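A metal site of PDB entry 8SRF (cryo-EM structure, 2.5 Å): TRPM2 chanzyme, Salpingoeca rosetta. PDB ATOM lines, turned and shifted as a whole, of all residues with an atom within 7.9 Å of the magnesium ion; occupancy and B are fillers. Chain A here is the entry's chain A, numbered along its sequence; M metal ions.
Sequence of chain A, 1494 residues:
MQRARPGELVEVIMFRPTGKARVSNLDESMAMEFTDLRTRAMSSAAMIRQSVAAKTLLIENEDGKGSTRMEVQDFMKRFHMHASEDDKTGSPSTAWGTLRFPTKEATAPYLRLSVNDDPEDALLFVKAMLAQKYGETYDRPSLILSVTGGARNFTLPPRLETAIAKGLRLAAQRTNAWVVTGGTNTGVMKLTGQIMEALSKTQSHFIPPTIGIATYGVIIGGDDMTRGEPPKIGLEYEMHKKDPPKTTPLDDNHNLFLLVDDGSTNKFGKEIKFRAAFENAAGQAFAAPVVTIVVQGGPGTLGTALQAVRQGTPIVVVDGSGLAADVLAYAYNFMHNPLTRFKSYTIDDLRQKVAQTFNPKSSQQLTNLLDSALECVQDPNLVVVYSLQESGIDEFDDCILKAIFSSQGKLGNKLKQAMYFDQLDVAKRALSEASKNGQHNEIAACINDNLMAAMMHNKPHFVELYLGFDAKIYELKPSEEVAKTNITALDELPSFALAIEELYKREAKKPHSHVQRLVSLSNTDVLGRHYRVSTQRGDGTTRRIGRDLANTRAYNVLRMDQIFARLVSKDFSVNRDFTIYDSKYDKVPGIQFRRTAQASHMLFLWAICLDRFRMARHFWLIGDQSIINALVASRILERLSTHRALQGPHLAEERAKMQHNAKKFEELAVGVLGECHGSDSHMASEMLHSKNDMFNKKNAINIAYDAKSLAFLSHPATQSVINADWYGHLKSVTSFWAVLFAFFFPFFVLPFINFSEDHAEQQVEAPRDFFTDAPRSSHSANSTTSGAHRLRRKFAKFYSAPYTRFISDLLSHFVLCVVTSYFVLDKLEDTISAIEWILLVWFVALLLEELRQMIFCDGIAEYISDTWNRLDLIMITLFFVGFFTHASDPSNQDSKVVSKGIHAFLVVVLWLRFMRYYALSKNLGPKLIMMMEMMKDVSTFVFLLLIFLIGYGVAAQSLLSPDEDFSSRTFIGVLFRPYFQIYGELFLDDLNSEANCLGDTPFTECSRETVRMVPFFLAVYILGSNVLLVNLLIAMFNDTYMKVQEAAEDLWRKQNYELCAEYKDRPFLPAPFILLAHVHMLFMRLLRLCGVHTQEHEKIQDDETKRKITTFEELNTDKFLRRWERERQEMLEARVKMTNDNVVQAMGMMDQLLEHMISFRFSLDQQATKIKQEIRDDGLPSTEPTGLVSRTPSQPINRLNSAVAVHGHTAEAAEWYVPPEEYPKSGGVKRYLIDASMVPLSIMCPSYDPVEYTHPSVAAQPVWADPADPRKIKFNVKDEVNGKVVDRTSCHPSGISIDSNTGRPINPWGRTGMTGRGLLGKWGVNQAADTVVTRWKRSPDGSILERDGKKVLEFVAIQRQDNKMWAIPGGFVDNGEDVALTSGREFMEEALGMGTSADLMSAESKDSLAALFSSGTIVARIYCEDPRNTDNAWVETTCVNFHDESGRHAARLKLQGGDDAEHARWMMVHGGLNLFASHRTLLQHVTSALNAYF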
ATOM      1  N   PHE A 593     -13.830  12.505  26.861  1.00  0.00           N
ATOM      2  CA  PHE A 593     -12.481  12.919  27.237  1.00  0.00           C
ATOM      3  C   PHE A 593     -12.485  13.725  28.527  1.00  0.00           C
ATOM      4  O   PHE A 593     -11.574  13.541  29.340  1.00  0.00           O
ATOM      5  CB  PHE A 593     -11.868  13.714  26.077  1.00  0.00           C
ATOM      6  CG  PHE A 593     -10.531  14.294  26.376  1.00  0.00           C
ATOM      7  CD1 PHE A 593      -9.447  13.450  26.717  1.00  0.00           C
ATOM      8  CD2 PHE A 593     -10.322  15.678  26.285  1.00  0.00           C
ATOM      9  CE1 PHE A 593      -8.184  13.988  26.984  1.00  0.00           C
ATOM     10  CE2 PHE A 593      -9.068  16.236  26.545  1.00  0.00           C
ATOM     11  CZ  PHE A 593      -7.994  15.383  26.891  1.00  0.00           C
ATOM     12  N   ALA A 597     -10.820  12.803  31.977  1.00  0.00           N
ATOM     13  CA  ALA A 597      -9.726  13.678  32.391  1.00  0.00           C
ATOM     14  C   ALA A 597      -9.897  14.120  33.843  1.00  0.00           C
ATOM     15  O   ALA A 597      -8.933  14.056  34.625  1.00  0.00           O
ATOM     16  CB  ALA A 597      -9.636  14.894  31.468  1.00  0.00           C
ATOM     17  N   SER A 600      -9.765  10.928  36.257  1.00  0.00           N
ATOM     18  CA  SER A 600      -8.341  10.557  36.310  1.00  0.00           C
ATOM     19  C   SER A 600      -7.561  11.498  37.204  1.00  0.00           C
ATOM     20  O   SER A 600      -6.624  11.050  37.863  1.00  0.00           O
ATOM     21  CB  SER A 600      -7.740  10.561  34.922  1.00  0.00           C
ATOM     22  OG  SER A 600      -7.734  11.869  34.464  1.00  0.00           O
ATOM     23  N   HIS A 618       0.077   6.159  35.808  1.00  0.00           N
ATOM     24  CA  HIS A 618      -0.989   5.657  34.928  1.00  0.00           C
ATOM     25  C   HIS A 618      -2.174   6.632  34.828  1.00  0.00           C
ATOM     26  O   HIS A 618      -2.677   6.875  33.710  1.00  0.00           O
ATOM     27  CB  HIS A 618      -1.469   4.277  35.341  1.00  0.00           C
ATOM     28  CG  HIS A 618      -2.477   3.714  34.389  1.00  0.00           C
ATOM     29  ND1 HIS A 618      -2.145   3.336  33.111  1.00  0.00           N
ATOM     30  CD2 HIS A 618      -3.812   3.522  34.507  1.00  0.00           C
ATOM     31  CE1 HIS A 618      -3.223   2.914  32.475  1.00  0.00           C
ATOM     32  NE2 HIS A 618      -4.244   3.010  33.302  1.00  0.00           N
ATOM     33  N   PHE A 619      -2.617   7.192  35.980  1.00  0.00           N
ATOM     34  CA  PHE A 619      -3.701   8.181  35.969  1.00  0.00           C
ATOM     35  C   PHE A 619      -3.255   9.507  35.366  1.00  0.00           C
ATOM     36  O   PHE A 619      -4.086  10.252  34.846  1.00  0.00           O
ATOM     37  CB  PHE A 619      -4.331   8.423  37.344  1.00  0.00           C
ATOM     38  CG  PHE A 619      -5.058   7.233  37.916  1.00  0.00           C
ATOM     39  CD1 PHE A 619      -5.990   6.556  37.117  1.00  0.00           C
ATOM     40  CD2 PHE A 619      -4.951   6.907  39.271  1.00  0.00           C
ATOM     41  CE1 PHE A 619      -6.713   5.470  37.621  1.00  0.00           C
ATOM     42  CE2 PHE A 619      -5.671   5.830  39.803  1.00  0.00           C
ATOM     43  CZ  PHE A 619      -6.549   5.115  38.968  1.00  0.00           C
ATOM     44  N   TRP A 620      -1.972   9.846  35.527  1.00  0.00           N
ATOM     45  CA  TRP A 620      -1.360  10.999  34.879  1.00  0.00           C
ATOM     46  C   TRP A 620      -1.339  10.832  33.364  1.00  0.00           C
ATOM     47  O   TRP A 620      -1.555  11.802  32.626  1.00  0.00           O
ATOM     48  CB  TRP A 620       0.045  11.192  35.451  1.00  0.00           C
ATOM     49  CG  TRP A 620       0.912  12.176  34.725  1.00  0.00           C
ATOM     50  CD1 TRP A 620       0.868  13.532  34.845  1.00  0.00           C
ATOM     51  CD2 TRP A 620       1.946  11.888  33.789  1.00  0.00           C
ATOM     52  NE1 TRP A 620       1.813  14.113  34.037  1.00  0.00           N
ATOM     53  CE2 TRP A 620       2.494  13.119  33.372  1.00  0.00           C
ATOM     54  CE3 TRP A 620       2.467  10.693  33.246  1.00  0.00           C
ATOM     55  CZ2 TRP A 620       3.538  13.205  32.444  1.00  0.00           C
ATOM     56  CZ3 TRP A 620       3.504  10.779  32.327  1.00  0.00           C
ATOM     57  CH2 TRP A 620       4.020  12.029  31.936  1.00  0.00           C
ATOM     58  N   LEU A 621      -1.031   9.610  32.873  1.00  0.00           N
ATOM     59  CA  LEU A 621      -1.026   9.345  31.429  1.00  0.00           C
ATOM     60  C   LEU A 621      -2.402   9.365  30.762  1.00  0.00           C
ATOM     61  O   LEU A 621      -2.501   9.836  29.619  1.00  0.00           O
ATOM     62  CB  LEU A 621      -0.348   7.980  31.197  1.00  0.00           C
ATOM     63  CG  LEU A 621      -0.336   7.250  29.841  1.00  0.00           C
ATOM     64  CD1 LEU A 621       0.257   8.020  28.677  1.00  0.00           C
ATOM     65  CD2 LEU A 621       0.365   5.901  30.002  1.00  0.00           C
ATOM     66  N   ILE A 622      -3.444   8.801  31.410  1.00  0.00           N
ATOM     67  CA  ILE A 622      -4.797   8.815  30.810  1.00  0.00           C
ATOM     68  C   ILE A 622      -5.425  10.213  30.693  1.00  0.00           C
ATOM     69  O   ILE A 622      -6.016  10.520  29.650  1.00  0.00           O
ATOM     70  CB  ILE A 622      -5.777   7.785  31.424  1.00  0.00           C
ATOM     71  CG1 ILE A 622      -5.930   7.897  32.926  1.00  0.00           C
ATOM     72  CG2 ILE A 622      -5.348   6.368  30.966  1.00  0.00           C
ATOM     73  CD1 ILE A 622      -6.850   6.861  33.535  1.00  0.00           C
ATOM     74  N   GLY A 623      -5.299  11.055  31.719  1.00  0.00           N
ATOM     75  CA  GLY A 623      -5.867  12.384  31.732  1.00  0.00           C
ATOM     76  C   GLY A 623      -5.074  13.403  30.940  1.00  0.00           C
ATOM     77  O   GLY A 623      -4.157  13.082  30.190  1.00  0.00           O
ATOM     78  N   ASP A 624      -5.429  14.676  31.136  1.00  0.00           N
ATOM     79  CA  ASP A 624      -4.730  15.729  30.412  1.00  0.00           C
ATOM     80  C   ASP A 624      -3.952  16.638  31.354  1.00  0.00           C
ATOM     81  O   ASP A 624      -3.932  16.411  32.573  1.00  0.00           O
ATOM     82  CB  ASP A 624      -5.714  16.506  29.529  1.00  0.00           C
ATOM     83  CG  ASP A 624      -6.675  17.438  30.295  1.00  0.00           C
ATOM     84  OD1 ASP A 624      -7.070  17.183  31.465  1.00  0.00           O
ATOM     85  OD2 ASP A 624      -7.046  18.475  29.707  1.00  0.00           O
ATOM     86  N   GLN A 625      -3.372  17.687  30.728  1.00  0.00           N
ATOM     87  CA  GLN A 625      -2.517  18.726  31.320  1.00  0.00           C
ATOM     88  C   GLN A 625      -1.316  18.090  32.033  1.00  0.00           C
ATOM     89  O   GLN A 625      -1.105  18.325  33.225  1.00  0.00           O
ATOM     90  CB  GLN A 625      -3.292  19.668  32.264  1.00  0.00           C
ATOM     91  CG  GLN A 625      -4.147  20.691  31.550  1.00  0.00           C
ATOM     92  CD  GLN A 625      -3.332  21.645  30.710  1.00  0.00           C
ATOM     93  OE1 GLN A 625      -2.287  22.134  31.135  1.00  0.00           O
ATOM     94  NE2 GLN A 625      -3.814  21.920  29.496  1.00  0.00           N
ATOM     95  N   SER A 626      -0.559  17.278  31.257  1.00  0.00           N
ATOM     96  CA  SER A 626       0.481  16.351  31.725  1.00  0.00           C
ATOM     97  C   SER A 626       1.653  17.035  32.429  1.00  0.00           C
ATOM     98  O   SER A 626       2.139  16.533  33.461  1.00  0.00           O
ATOM     99  CB  SER A 626       0.994  15.519  30.540  1.00  0.00           C
ATOM    100  OG  SER A 626      -0.053  14.801  29.916  1.00  0.00           O
ATOM    101  N   THR A1110      -3.630  21.510  23.557  1.00  0.00           N
ATOM    102  CA  THR A1110      -4.005  20.314  24.330  1.00  0.00           C
ATOM    103  C   THR A1110      -3.719  19.005  23.569  1.00  0.00           C
ATOM    104  O   THR A1110      -3.118  18.072  24.134  1.00  0.00           O
ATOM    105  CB  THR A1110      -5.492  20.433  24.709  1.00  0.00           C
ATOM    106  OG1 THR A1110      -5.665  21.551  25.584  1.00  0.00           O
ATOM    107  CG2 THR A1110      -6.027  19.188  25.410  1.00  0.00           C
ATOM    108  N   GLU A1113       0.124  18.611  23.207  1.00  0.00           N
ATOM    109  CA  GLU A1113       0.702  18.190  24.487  1.00  0.00           C
ATOM    110  C   GLU A1113       0.457  16.705  24.759  1.00  0.00           C
ATOM    111  O   GLU A1113       1.364  16.010  25.236  1.00  0.00           O
ATOM    112  CB  GLU A1113       0.120  19.065  25.609  1.00  0.00           C
ATOM    113  CG  GLU A1113       0.623  18.778  27.012  1.00  0.00           C
ATOM    114  CD  GLU A1113       0.119  19.779  28.035  1.00  0.00           C
ATOM    115  OE1 GLU A1113      -0.875  20.481  27.730  1.00  0.00           O
ATOM    116  OE2 GLU A1113       0.698  19.861  29.134  1.00  0.00           O
ATOM    117  N   GLU A1114      -0.764  16.206  24.438  1.00  0.00           N
ATOM    118  CA  GLU A1114      -1.108  14.785  24.588  1.00  0.00           C
ATOM    119  C   GLU A1114      -0.324  13.893  23.629  1.00  0.00           C
ATOM    120  O   GLU A1114       0.107  12.794  24.035  1.00  0.00           O
ATOM    121  CB  GLU A1114      -2.611  14.544  24.454  1.00  0.00           C
ATOM    122  CG  GLU A1114      -3.313  15.070  25.648  1.00  0.00           C
ATOM    123  CD  GLU A1114      -3.074  14.156  26.829  1.00  0.00           C
ATOM    124  OE1 GLU A1114      -3.053  12.923  26.661  1.00  0.00           O
ATOM    125  OE2 GLU A1114      -2.739  14.673  27.900  1.00  0.00           O
ATOM    126  N   LEU A1115      -0.188  14.339  22.361  1.00  0.00           N
ATOM    127  CA  LEU A1115       0.571  13.632  21.328  1.00  0.00           C
ATOM    128  C   LEU A1115       2.053  13.536  21.708  1.00  0.00           C
ATOM    129  O   LEU A1115       2.651  12.454  21.602  1.00  0.00           O
ATOM    130  CB  LEU A1115       0.407  14.345  19.982  1.00  0.00           C
ATOM    131  CG  LEU A1115       1.184  13.786  18.792  1.00  0.00           C
ATOM    132  CD1 LEU A1115       0.488  12.572  18.225  1.00  0.00           C
ATOM    133  CD2 LEU A1115       1.376  14.849  17.727  1.00  0.00           C
ATOM    134  N   THR A1117       3.214  13.807  24.825  1.00  0.00           N
ATOM    135  CA  THR A1117       3.243  12.964  26.027  1.00  0.00           C
ATOM    136  C   THR A1117       3.357  11.487  25.656  1.00  0.00           C
ATOM    137  O   THR A1117       4.179  10.751  26.244  1.00  0.00           O
ATOM    138  CB  THR A1117       1.998  13.230  26.868  1.00  0.00           C
ATOM    139  OG1 THR A1117       1.897  14.637  27.133  1.00  0.00           O
ATOM    140  CG2 THR A1117       2.048  12.500  28.202  1.00  0.00           C
ATOM    141  N   ASP A1118       2.517  11.047  24.686  1.00  0.00           N
ATOM    142  CA  ASP A1118       2.556   9.676  24.150  1.00  0.00           C
ATOM    143  C   ASP A1118       3.884   9.374  23.446  1.00  0.00           C
ATOM    144  O   ASP A1118       4.407   8.255  23.569  1.00  0.00           O
ATOM    145  CB  ASP A1118       1.389   9.398  23.203  1.00  0.00           C
ATOM    146  CG  ASP A1118       0.040   9.571  23.861  1.00  0.00           C
ATOM    147  OD1 ASP A1118      -0.142   9.066  24.993  1.00  0.00           O
ATOM    148  OD2 ASP A1118      -0.870  10.111  23.214  1.00  0.00           O
HETATM  149 MG    MG M   1      -3.109  12.056  28.610  1.00  0.00          MG
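The side-chain hydroxyl (OG) of Ser 626 sits at hydrogen-bond distance from the side-chain carboxylate (OE2) of Glu 1114, at 3.4 Å.
The magnesium ion is bound by OE1 of Glu 1114 (2.1 Å), O of Gly 623 (2.2 Å) and O of Leu 621 (2.5 Å).
The magnesium ion has three donor atoms within binding distance.
Slightly farther from the magnesium ion lies OE2 of Glu 1114 (2.7 Å).
Residues that only touch the magnesium ion: Ile 622 (3.4 Å).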
